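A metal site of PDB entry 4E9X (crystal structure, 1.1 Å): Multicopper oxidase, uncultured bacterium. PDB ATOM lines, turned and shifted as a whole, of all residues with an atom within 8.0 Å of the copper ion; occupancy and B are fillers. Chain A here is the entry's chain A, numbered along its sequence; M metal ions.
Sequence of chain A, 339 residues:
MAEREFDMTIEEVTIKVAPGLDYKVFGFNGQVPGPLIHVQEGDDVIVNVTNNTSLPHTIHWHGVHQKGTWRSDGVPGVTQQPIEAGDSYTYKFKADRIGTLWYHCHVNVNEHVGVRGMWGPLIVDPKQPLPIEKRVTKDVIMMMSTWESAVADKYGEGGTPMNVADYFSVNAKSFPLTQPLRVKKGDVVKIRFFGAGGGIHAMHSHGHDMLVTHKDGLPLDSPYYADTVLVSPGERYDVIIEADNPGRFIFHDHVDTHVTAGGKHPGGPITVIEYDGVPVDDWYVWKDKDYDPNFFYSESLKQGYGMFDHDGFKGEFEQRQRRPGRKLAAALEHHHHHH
The side-chain sulfur (SG) of Cys 105 lies close to the backbone NH (N) of Val 107 (3.3 Å).
N of Thr 58 sits close to SG of Cys 105 (3.5 Å).
ND1 of His 112 lies close to O of Val 107.
NE2 of His 57 sits close to O of Leu 55, 3.3 Å away.
The backbone carbonyl oxygen (O) of His 57 sits at hydrogen-bond distance from the backbone NH (N) of Ile 83, at 2.8 Å.
NE2 of His 57 lies within hydrogen-bond range of OG1 of Thr 53, at 2.8 Å.
Residues that only touch the copper ion: Pro 56 and Val 107.
Within 4 Å of the copper ion: Pro 56, His 57, Cys 105, Val 107, His 112 and Met 118.
Along chain A the residues within 4 Å of the copper ion span positions 56 to 118.
The copper ion is bound by a ring nitrogen (ND1) of His 112 (2.0 Å), a ring nitrogen (ND1) of His 57 (2.0 Å), the side-chain sulfur (SG) of Cys 105 (2.2 Å) and the side-chain sulfur (SD) of Met 118 (2.8 Å).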
ATOM      1  N   ILE A  10       8.532 -26.451  -3.201  1.00  0.00           N
ATOM      2  CA  ILE A  10       8.080 -25.895  -4.450  1.00  0.00           C
ATOM      3  C   ILE A  10       9.344 -25.456  -5.202  1.00  0.00           C
ATOM      4  O   ILE A  10      10.098 -24.684  -4.567  1.00  0.00           O
ATOM      5  CB  ILE A  10       7.078 -24.745  -4.343  1.00  0.00           C
ATOM      6  CG1 ILE A  10       5.980 -25.016  -3.306  1.00  0.00           C
ATOM      7  CG2 ILE A  10       6.429 -24.477  -5.700  1.00  0.00           C
ATOM      8  CD1 ILE A  10       5.037 -23.833  -3.118  1.00  0.00           C
ATOM      9  N   PHE A  26       6.536 -24.695 -11.912  1.00  0.00           N
ATOM     10  CA  PHE A  26       6.748 -24.639 -10.478  1.00  0.00           C
ATOM     11  C   PHE A  26       6.344 -25.990  -9.903  1.00  0.00           C
ATOM     12  O   PHE A  26       5.209 -26.210  -9.529  1.00  0.00           O
ATOM     13  CB  PHE A  26       5.918 -23.512  -9.865  1.00  0.00           C
ATOM     14  CG  PHE A  26       6.309 -22.103 -10.294  1.00  0.00           C
ATOM     15  CD1 PHE A  26       7.593 -21.610 -10.092  1.00  0.00           C
ATOM     16  CD2 PHE A  26       5.347 -21.293 -10.893  1.00  0.00           C
ATOM     17  CE1 PHE A  26       7.922 -20.296 -10.455  1.00  0.00           C
ATOM     18  CE2 PHE A  26       5.674 -20.001 -11.263  1.00  0.00           C
ATOM     19  CZ  PHE A  26       6.958 -19.516 -11.021  1.00  0.00           C
ATOM     20  N   PHE A  28       5.948 -29.080  -7.492  1.00  0.00           N
ATOM     21  CA  PHE A  28       5.987 -29.598  -6.141  1.00  0.00           C
ATOM     22  C   PHE A  28       7.041 -30.714  -6.107  1.00  0.00           C
ATOM     23  O   PHE A  28       7.022 -31.627  -6.936  1.00  0.00           O
ATOM     24  CB  PHE A  28       4.606 -30.112  -5.740  1.00  0.00           C
ATOM     25  CG  PHE A  28       3.568 -28.985  -5.554  1.00  0.00           C
ATOM     26  CD1 PHE A  28       3.764 -28.027  -4.571  1.00  0.00           C
ATOM     27  CD2 PHE A  28       2.469 -28.908  -6.369  1.00  0.00           C
ATOM     28  CE1 PHE A  28       2.865 -26.965  -4.374  1.00  0.00           C
ATOM     29  CE2 PHE A  28       1.558 -27.902  -6.156  1.00  0.00           C
ATOM     30  CZ  PHE A  28       1.722 -26.922  -5.144  1.00  0.00           C
ATOM     31  N   ASN A  51       8.651 -22.851   0.077  1.00  0.00           N
ATOM     32  CA  ASN A  51       8.652 -22.263  -1.269  1.00  0.00           C
ATOM     33  C   ASN A  51      10.068 -21.917  -1.715  1.00  0.00           C
ATOM     34  O   ASN A  51      10.600 -20.869  -1.288  1.00  0.00           O
ATOM     35  CB  ASN A  51       7.771 -20.990  -1.218  1.00  0.00           C
ATOM     36  CG  ASN A  51       7.662 -20.300  -2.565  1.00  0.00           C
ATOM     37  OD1 ASN A  51       8.286 -20.778  -3.532  1.00  0.00           O
ATOM     38  ND2 ASN A  51       6.873 -19.245  -2.629  1.00  0.00           N
ATOM     39  N   THR A  53      10.904 -21.074  -4.717  1.00  0.00           N
ATOM     40  CA  THR A  53      10.796 -20.364  -6.010  1.00  0.00           C
ATOM     41  C   THR A  53      10.835 -18.854  -5.752  1.00  0.00           C
ATOM     42  O   THR A  53      10.918 -18.435  -4.590  1.00  0.00           O
ATOM     43  CB  THR A  53       9.523 -20.704  -6.799  1.00  0.00           C
ATOM     44  OG1 THR A  53       8.414 -19.942  -6.224  1.00  0.00           O
ATOM     45  CG2 THR A  53       9.175 -22.167  -6.683  1.00  0.00           C
ATOM     46  N   LEU A  55       8.425 -16.734  -6.550  1.00  0.00           N
ATOM     47  CA  LEU A  55       7.089 -16.136  -6.584  1.00  0.00           C
ATOM     48  C   LEU A  55       6.266 -16.737  -5.450  1.00  0.00           C
ATOM     49  O   LEU A  55       6.563 -17.837  -4.975  1.00  0.00           O
ATOM     50  CB  LEU A  55       6.385 -16.440  -7.896  1.00  0.00           C
ATOM     51  CG  LEU A  55       6.885 -15.787  -9.185  1.00  0.00           C
ATOM     52  CD1 LEU A  55       6.049 -16.126 -10.393  1.00  0.00           C
ATOM     53  CD2 LEU A  55       6.877 -14.263  -8.984  1.00  0.00           C
ATOM     54  N   PRO A  56       5.217 -16.046  -4.981  1.00  0.00           N
ATOM     55  CA  PRO A  56       4.368 -16.579  -3.962  1.00  0.00           C
ATOM     56  C   PRO A  56       3.433 -17.687  -4.493  1.00  0.00           C
ATOM     57  O   PRO A  56       3.028 -17.708  -5.670  1.00  0.00           O
ATOM     58  CB  PRO A  56       3.532 -15.373  -3.518  1.00  0.00           C
ATOM     59  CG  PRO A  56       3.692 -14.367  -4.590  1.00  0.00           C
ATOM     60  CD  PRO A  56       4.907 -14.667  -5.395  1.00  0.00           C
ATOM     61  N   HIS A  57       3.120 -18.598  -3.545  1.00  0.00           N
ATOM     62  CA  HIS A  57       2.211 -19.720  -3.842  1.00  0.00           C
ATOM     63  C   HIS A  57       1.379 -20.036  -2.606  1.00  0.00           C
ATOM     64  O   HIS A  57       1.674 -19.539  -1.521  1.00  0.00           O
ATOM     65  CB  HIS A  57       3.023 -20.988  -4.204  1.00  0.00           C
ATOM     66  CG  HIS A  57       3.932 -20.788  -5.383  1.00  0.00           C
ATOM     67  ND1 HIS A  57       3.478 -20.660  -6.678  1.00  0.00           N
ATOM     68  CD2 HIS A  57       5.291 -20.658  -5.409  1.00  0.00           C
ATOM     69  CE1 HIS A  57       4.580 -20.472  -7.452  1.00  0.00           C
ATOM     70  NE2 HIS A  57       5.693 -20.462  -6.686  1.00  0.00           N
ATOM     71  N   THR A  58       0.412 -20.949  -2.769  1.00  0.00           N
ATOM     72  CA  THR A  58      -0.244 -21.630  -1.664  1.00  0.00           C
ATOM     73  C   THR A  58      -0.476 -23.093  -2.061  1.00  0.00           C
ATOM     74  O   THR A  58      -0.159 -23.426  -3.209  1.00  0.00           O
ATOM     75  CB  THR A  58      -1.614 -21.043  -1.279  1.00  0.00           C
ATOM     76  OG1 THR A  58      -2.473 -21.128  -2.443  1.00  0.00           O
ATOM     77  CG2 THR A  58      -1.532 -19.579  -0.837  1.00  0.00           C
ATOM     78  N   ILE A  59      -1.019 -23.898  -1.173  1.00  0.00           N
ATOM     79  CA  ILE A  59      -1.604 -25.165  -1.636  1.00  0.00           C
ATOM     80  C   ILE A  59      -3.042 -25.229  -1.133  1.00  0.00           C
ATOM     81  O   ILE A  59      -3.268 -25.162   0.078  1.00  0.00           O
ATOM     82  CB  ILE A  59      -0.829 -26.390  -1.166  1.00  0.00           C
ATOM     83  CG1 ILE A  59       0.681 -26.320  -1.492  1.00  0.00           C
ATOM     84  CG2 ILE A  59      -1.450 -27.657  -1.805  1.00  0.00           C
ATOM     85  CD1 ILE A  59       1.400 -27.651  -1.127  1.00  0.00           C
ATOM     86  N   ILE A  83       2.254 -17.799   0.545  1.00  0.00           N
ATOM     87  CA  ILE A  83       3.580 -18.209   0.991  1.00  0.00           C
ATOM     88  C   ILE A  83       4.592 -17.540   0.109  1.00  0.00           C
ATOM     89  O   ILE A  83       4.745 -17.859  -1.073  1.00  0.00           O
ATOM     90  CB  ILE A  83       3.724 -19.742   0.904  1.00  0.00           C
ATOM     91  CG1 ILE A  83       2.578 -20.501   1.571  1.00  0.00           C
ATOM     92  CG2 ILE A  83       5.095 -20.160   1.460  1.00  0.00           C
ATOM     93  CD1 ILE A  83       2.584 -21.999   1.231  1.00  0.00           C
ATOM     94  N   HIS A 104      -3.444 -28.237  -5.407  1.00  0.00           N
ATOM     95  CA  HIS A 104      -2.894 -27.356  -6.426  1.00  0.00           C
ATOM     96  C   HIS A 104      -2.671 -25.962  -5.844  1.00  0.00           C
ATOM     97  O   HIS A 104      -3.340 -25.605  -4.856  1.00  0.00           O
ATOM     98  CB  HIS A 104      -3.800 -27.251  -7.664  1.00  0.00           C
ATOM     99  CG  HIS A 104      -5.230 -26.797  -7.461  1.00  0.00           C
ATOM    100  ND1 HIS A 104      -5.608 -25.498  -7.292  1.00  0.00           N
ATOM    101  CD2 HIS A 104      -6.363 -27.527  -7.407  1.00  0.00           C
ATOM    102  CE1 HIS A 104      -6.944 -25.446  -7.146  1.00  0.00           C
ATOM    103  NE2 HIS A 104      -7.436 -26.668  -7.228  1.00  0.00           N
ATOM    104  N   CYS A 105      -1.814 -25.187  -6.481  1.00  0.00           N
ATOM    105  CA  CYS A 105      -1.673 -23.790  -6.011  1.00  0.00           C
ATOM    106  C   CYS A 105      -2.987 -23.063  -6.174  1.00  0.00           C
ATOM    107  O   CYS A 105      -3.776 -23.357  -7.070  1.00  0.00           O
ATOM    108  CB  CYS A 105      -0.549 -23.130  -6.845  1.00  0.00           C
ATOM    109  SG  CYS A 105      -0.149 -21.483  -6.225  1.00  0.00           S
ATOM    110  N   HIS A 106      -3.219 -22.047  -5.344  1.00  0.00           N
ATOM    111  CA  HIS A 106      -4.375 -21.178  -5.514  1.00  0.00           C
ATOM    112  C   HIS A 106      -4.005 -19.692  -5.637  1.00  0.00           C
ATOM    113  O   HIS A 106      -4.856 -18.826  -5.436  1.00  0.00           O
ATOM    114  CB  HIS A 106      -5.389 -21.415  -4.375  1.00  0.00           C
ATOM    115  CG  HIS A 106      -6.812 -21.426  -4.835  1.00  0.00           C
ATOM    116  ND1 HIS A 106      -7.446 -20.290  -5.266  1.00  0.00           N
ATOM    117  CD2 HIS A 106      -7.727 -22.428  -4.901  1.00  0.00           C
ATOM    118  CE1 HIS A 106      -8.680 -20.602  -5.604  1.00  0.00           C
ATOM    119  NE2 HIS A 106      -8.897 -21.882  -5.395  1.00  0.00           N
ATOM    120  N   VAL A 107      -2.753 -19.402  -5.976  1.00  0.00           N
ATOM    121  CA  VAL A 107      -2.267 -18.085  -6.326  1.00  0.00           C
ATOM    122  C   VAL A 107      -2.154 -18.032  -7.881  1.00  0.00           C
ATOM    123  O   VAL A 107      -1.621 -18.971  -8.492  1.00  0.00           O
ATOM    124  CB  VAL A 107      -0.882 -17.827  -5.727  1.00  0.00           C
ATOM    125  CG1 VAL A 107      -0.325 -16.509  -6.279  1.00  0.00           C
ATOM    126  CG2 VAL A 107      -0.898 -17.824  -4.217  1.00  0.00           C
ATOM    127  N   ASN A 108      -2.602 -16.934  -8.446  1.00  0.00           N
ATOM    128  CA  ASN A 108      -2.422 -16.733  -9.895  1.00  0.00           C
ATOM    129  C   ASN A 108      -2.836 -17.961 -10.690  1.00  0.00           C
ATOM    130  O   ASN A 108      -2.105 -18.462 -11.563  1.00  0.00           O
ATOM    131  CB  ASN A 108      -0.938 -16.368 -10.104  1.00  0.00           C
ATOM    132  CG  ASN A 108      -0.573 -14.947  -9.694  1.00  0.00           C
ATOM    133  OD1 ASN A 108      -1.498 -14.111  -9.566  1.00  0.00           O
ATOM    134  ND2 ASN A 108       0.683 -14.513  -9.492  1.00  0.00           N
ATOM    135  N   VAL A 109      -3.938 -18.591 -10.330  1.00  0.00           N
ATOM    136  CA  VAL A 109      -4.232 -19.948 -10.799  1.00  0.00           C
ATOM    137  C   VAL A 109      -4.303 -20.141 -12.310  1.00  0.00           C
ATOM    138  O   VAL A 109      -3.953 -21.219 -12.799  1.00  0.00           O
ATOM    139  CB  VAL A 109      -5.543 -20.487 -10.188  1.00  0.00           C
ATOM    140  CG1 VAL A 109      -5.417 -20.354  -8.660  1.00  0.00           C
ATOM    141  CG2 VAL A 109      -6.808 -19.850 -10.698  1.00  0.00           C
ATOM    142  N   GLU A 111      -2.405 -19.058 -14.482  1.00  0.00           N
ATOM    143  CA  GLU A 111      -1.075 -19.406 -14.950  1.00  0.00           C
ATOM    144  C   GLU A 111      -0.517 -20.575 -14.189  1.00  0.00           C
ATOM    145  O   GLU A 111       0.006 -21.549 -14.777  1.00  0.00           O
ATOM    146  CB  GLU A 111      -0.133 -18.186 -14.821  1.00  0.00           C
ATOM    147  CG  GLU A 111       1.270 -18.537 -15.300  1.00  0.00           C
ATOM    148  CD  GLU A 111       2.399 -17.607 -14.924  1.00  0.00           C
ATOM    149  OE1 GLU A 111       2.130 -16.514 -14.405  1.00  0.00           O
ATOM    150  OE2 GLU A 111       3.574 -18.045 -15.166  1.00  0.00           O
ATOM    151  N   HIS A 112      -0.538 -20.536 -12.827  1.00  0.00           N
ATOM    152  CA  HIS A 112       0.201 -21.527 -12.051  1.00  0.00           C
ATOM    153  C   HIS A 112      -0.394 -22.924 -12.229  1.00  0.00           C
ATOM    154  O   HIS A 112       0.365 -23.893 -12.331  1.00  0.00           O
ATOM    155  CB  HIS A 112       0.250 -21.086 -10.568  1.00  0.00           C
ATOM    156  CG  HIS A 112       1.181 -19.933 -10.319  1.00  0.00           C
ATOM    157  ND1 HIS A 112       1.670 -19.667  -9.038  1.00  0.00           N
ATOM    158  CD2 HIS A 112       1.665 -18.981 -11.172  1.00  0.00           C
ATOM    159  CE1 HIS A 112       2.436 -18.592  -9.116  1.00  0.00           C
ATOM    160  NE2 HIS A 112       2.450 -18.171 -10.376  1.00  0.00           N
ATOM    161  N   VAL A 113      -1.732 -23.022 -12.204  1.00  0.00           N
ATOM    162  CA  VAL A 113      -2.400 -24.297 -12.399  1.00  0.00           C
ATOM    163  C   VAL A 113      -2.557 -24.541 -13.883  1.00  0.00           C
ATOM    164  O   VAL A 113      -2.365 -25.674 -14.342  1.00  0.00           O
ATOM    165  CB  VAL A 113      -3.755 -24.390 -11.647  1.00  0.00           C
ATOM    166  CG1 VAL A 113      -4.421 -25.722 -11.898  1.00  0.00           C
ATOM    167  CG2 VAL A 113      -3.499 -24.150 -10.153  1.00  0.00           C
ATOM    168  N   ARG A 116       1.783 -24.047 -15.194  1.00  0.00           N
ATOM    169  CA  ARG A 116       3.030 -24.217 -14.470  1.00  0.00           C
ATOM    170  C   ARG A 116       3.040 -25.480 -13.638  1.00  0.00           C
ATOM    171  O   ARG A 116       3.942 -25.673 -12.820  1.00  0.00           O
ATOM    172  CB  ARG A 116       3.358 -22.991 -13.600  1.00  0.00           C
ATOM    173  CG  ARG A 116       3.487 -21.700 -14.391  1.00  0.00           C
ATOM    174  CD  ARG A 116       4.647 -21.680 -15.390  1.00  0.00           C
ATOM    175  NE  ARG A 116       4.460 -20.438 -16.204  1.00  0.00           N
ATOM    176  CZ  ARG A 116       4.991 -20.292 -17.397  1.00  0.00           C
ATOM    177  NH1 ARG A 116       5.827 -21.210 -17.956  1.00  0.00           N
ATOM    178  NH2 ARG A 116       4.709 -19.189 -18.102  1.00  0.00           N
ATOM    179  N   MET A 118       1.369 -26.812 -11.211  1.00  0.00           N
ATOM    180  CA  MET A 118       1.255 -26.819  -9.740  1.00  0.00           C
ATOM    181  C   MET A 118       0.067 -27.613  -9.257  1.00  0.00           C
ATOM    182  O   MET A 118      -0.921 -27.086  -8.726  1.00  0.00           O
ATOM    183  CB  MET A 118       1.136 -25.355  -9.247  1.00  0.00           C
ATOM    184  CG  MET A 118       2.366 -24.521  -9.722  1.00  0.00           C
ATOM    185  SD  MET A 118       2.656 -23.131  -8.601  1.00  0.00           S
ATOM    186  CE  MET A 118       3.205 -23.976  -7.110  1.00  0.00           C
HETATM  187 CU    CU M   1       1.611 -20.846  -7.425  1.00  0.00          CU
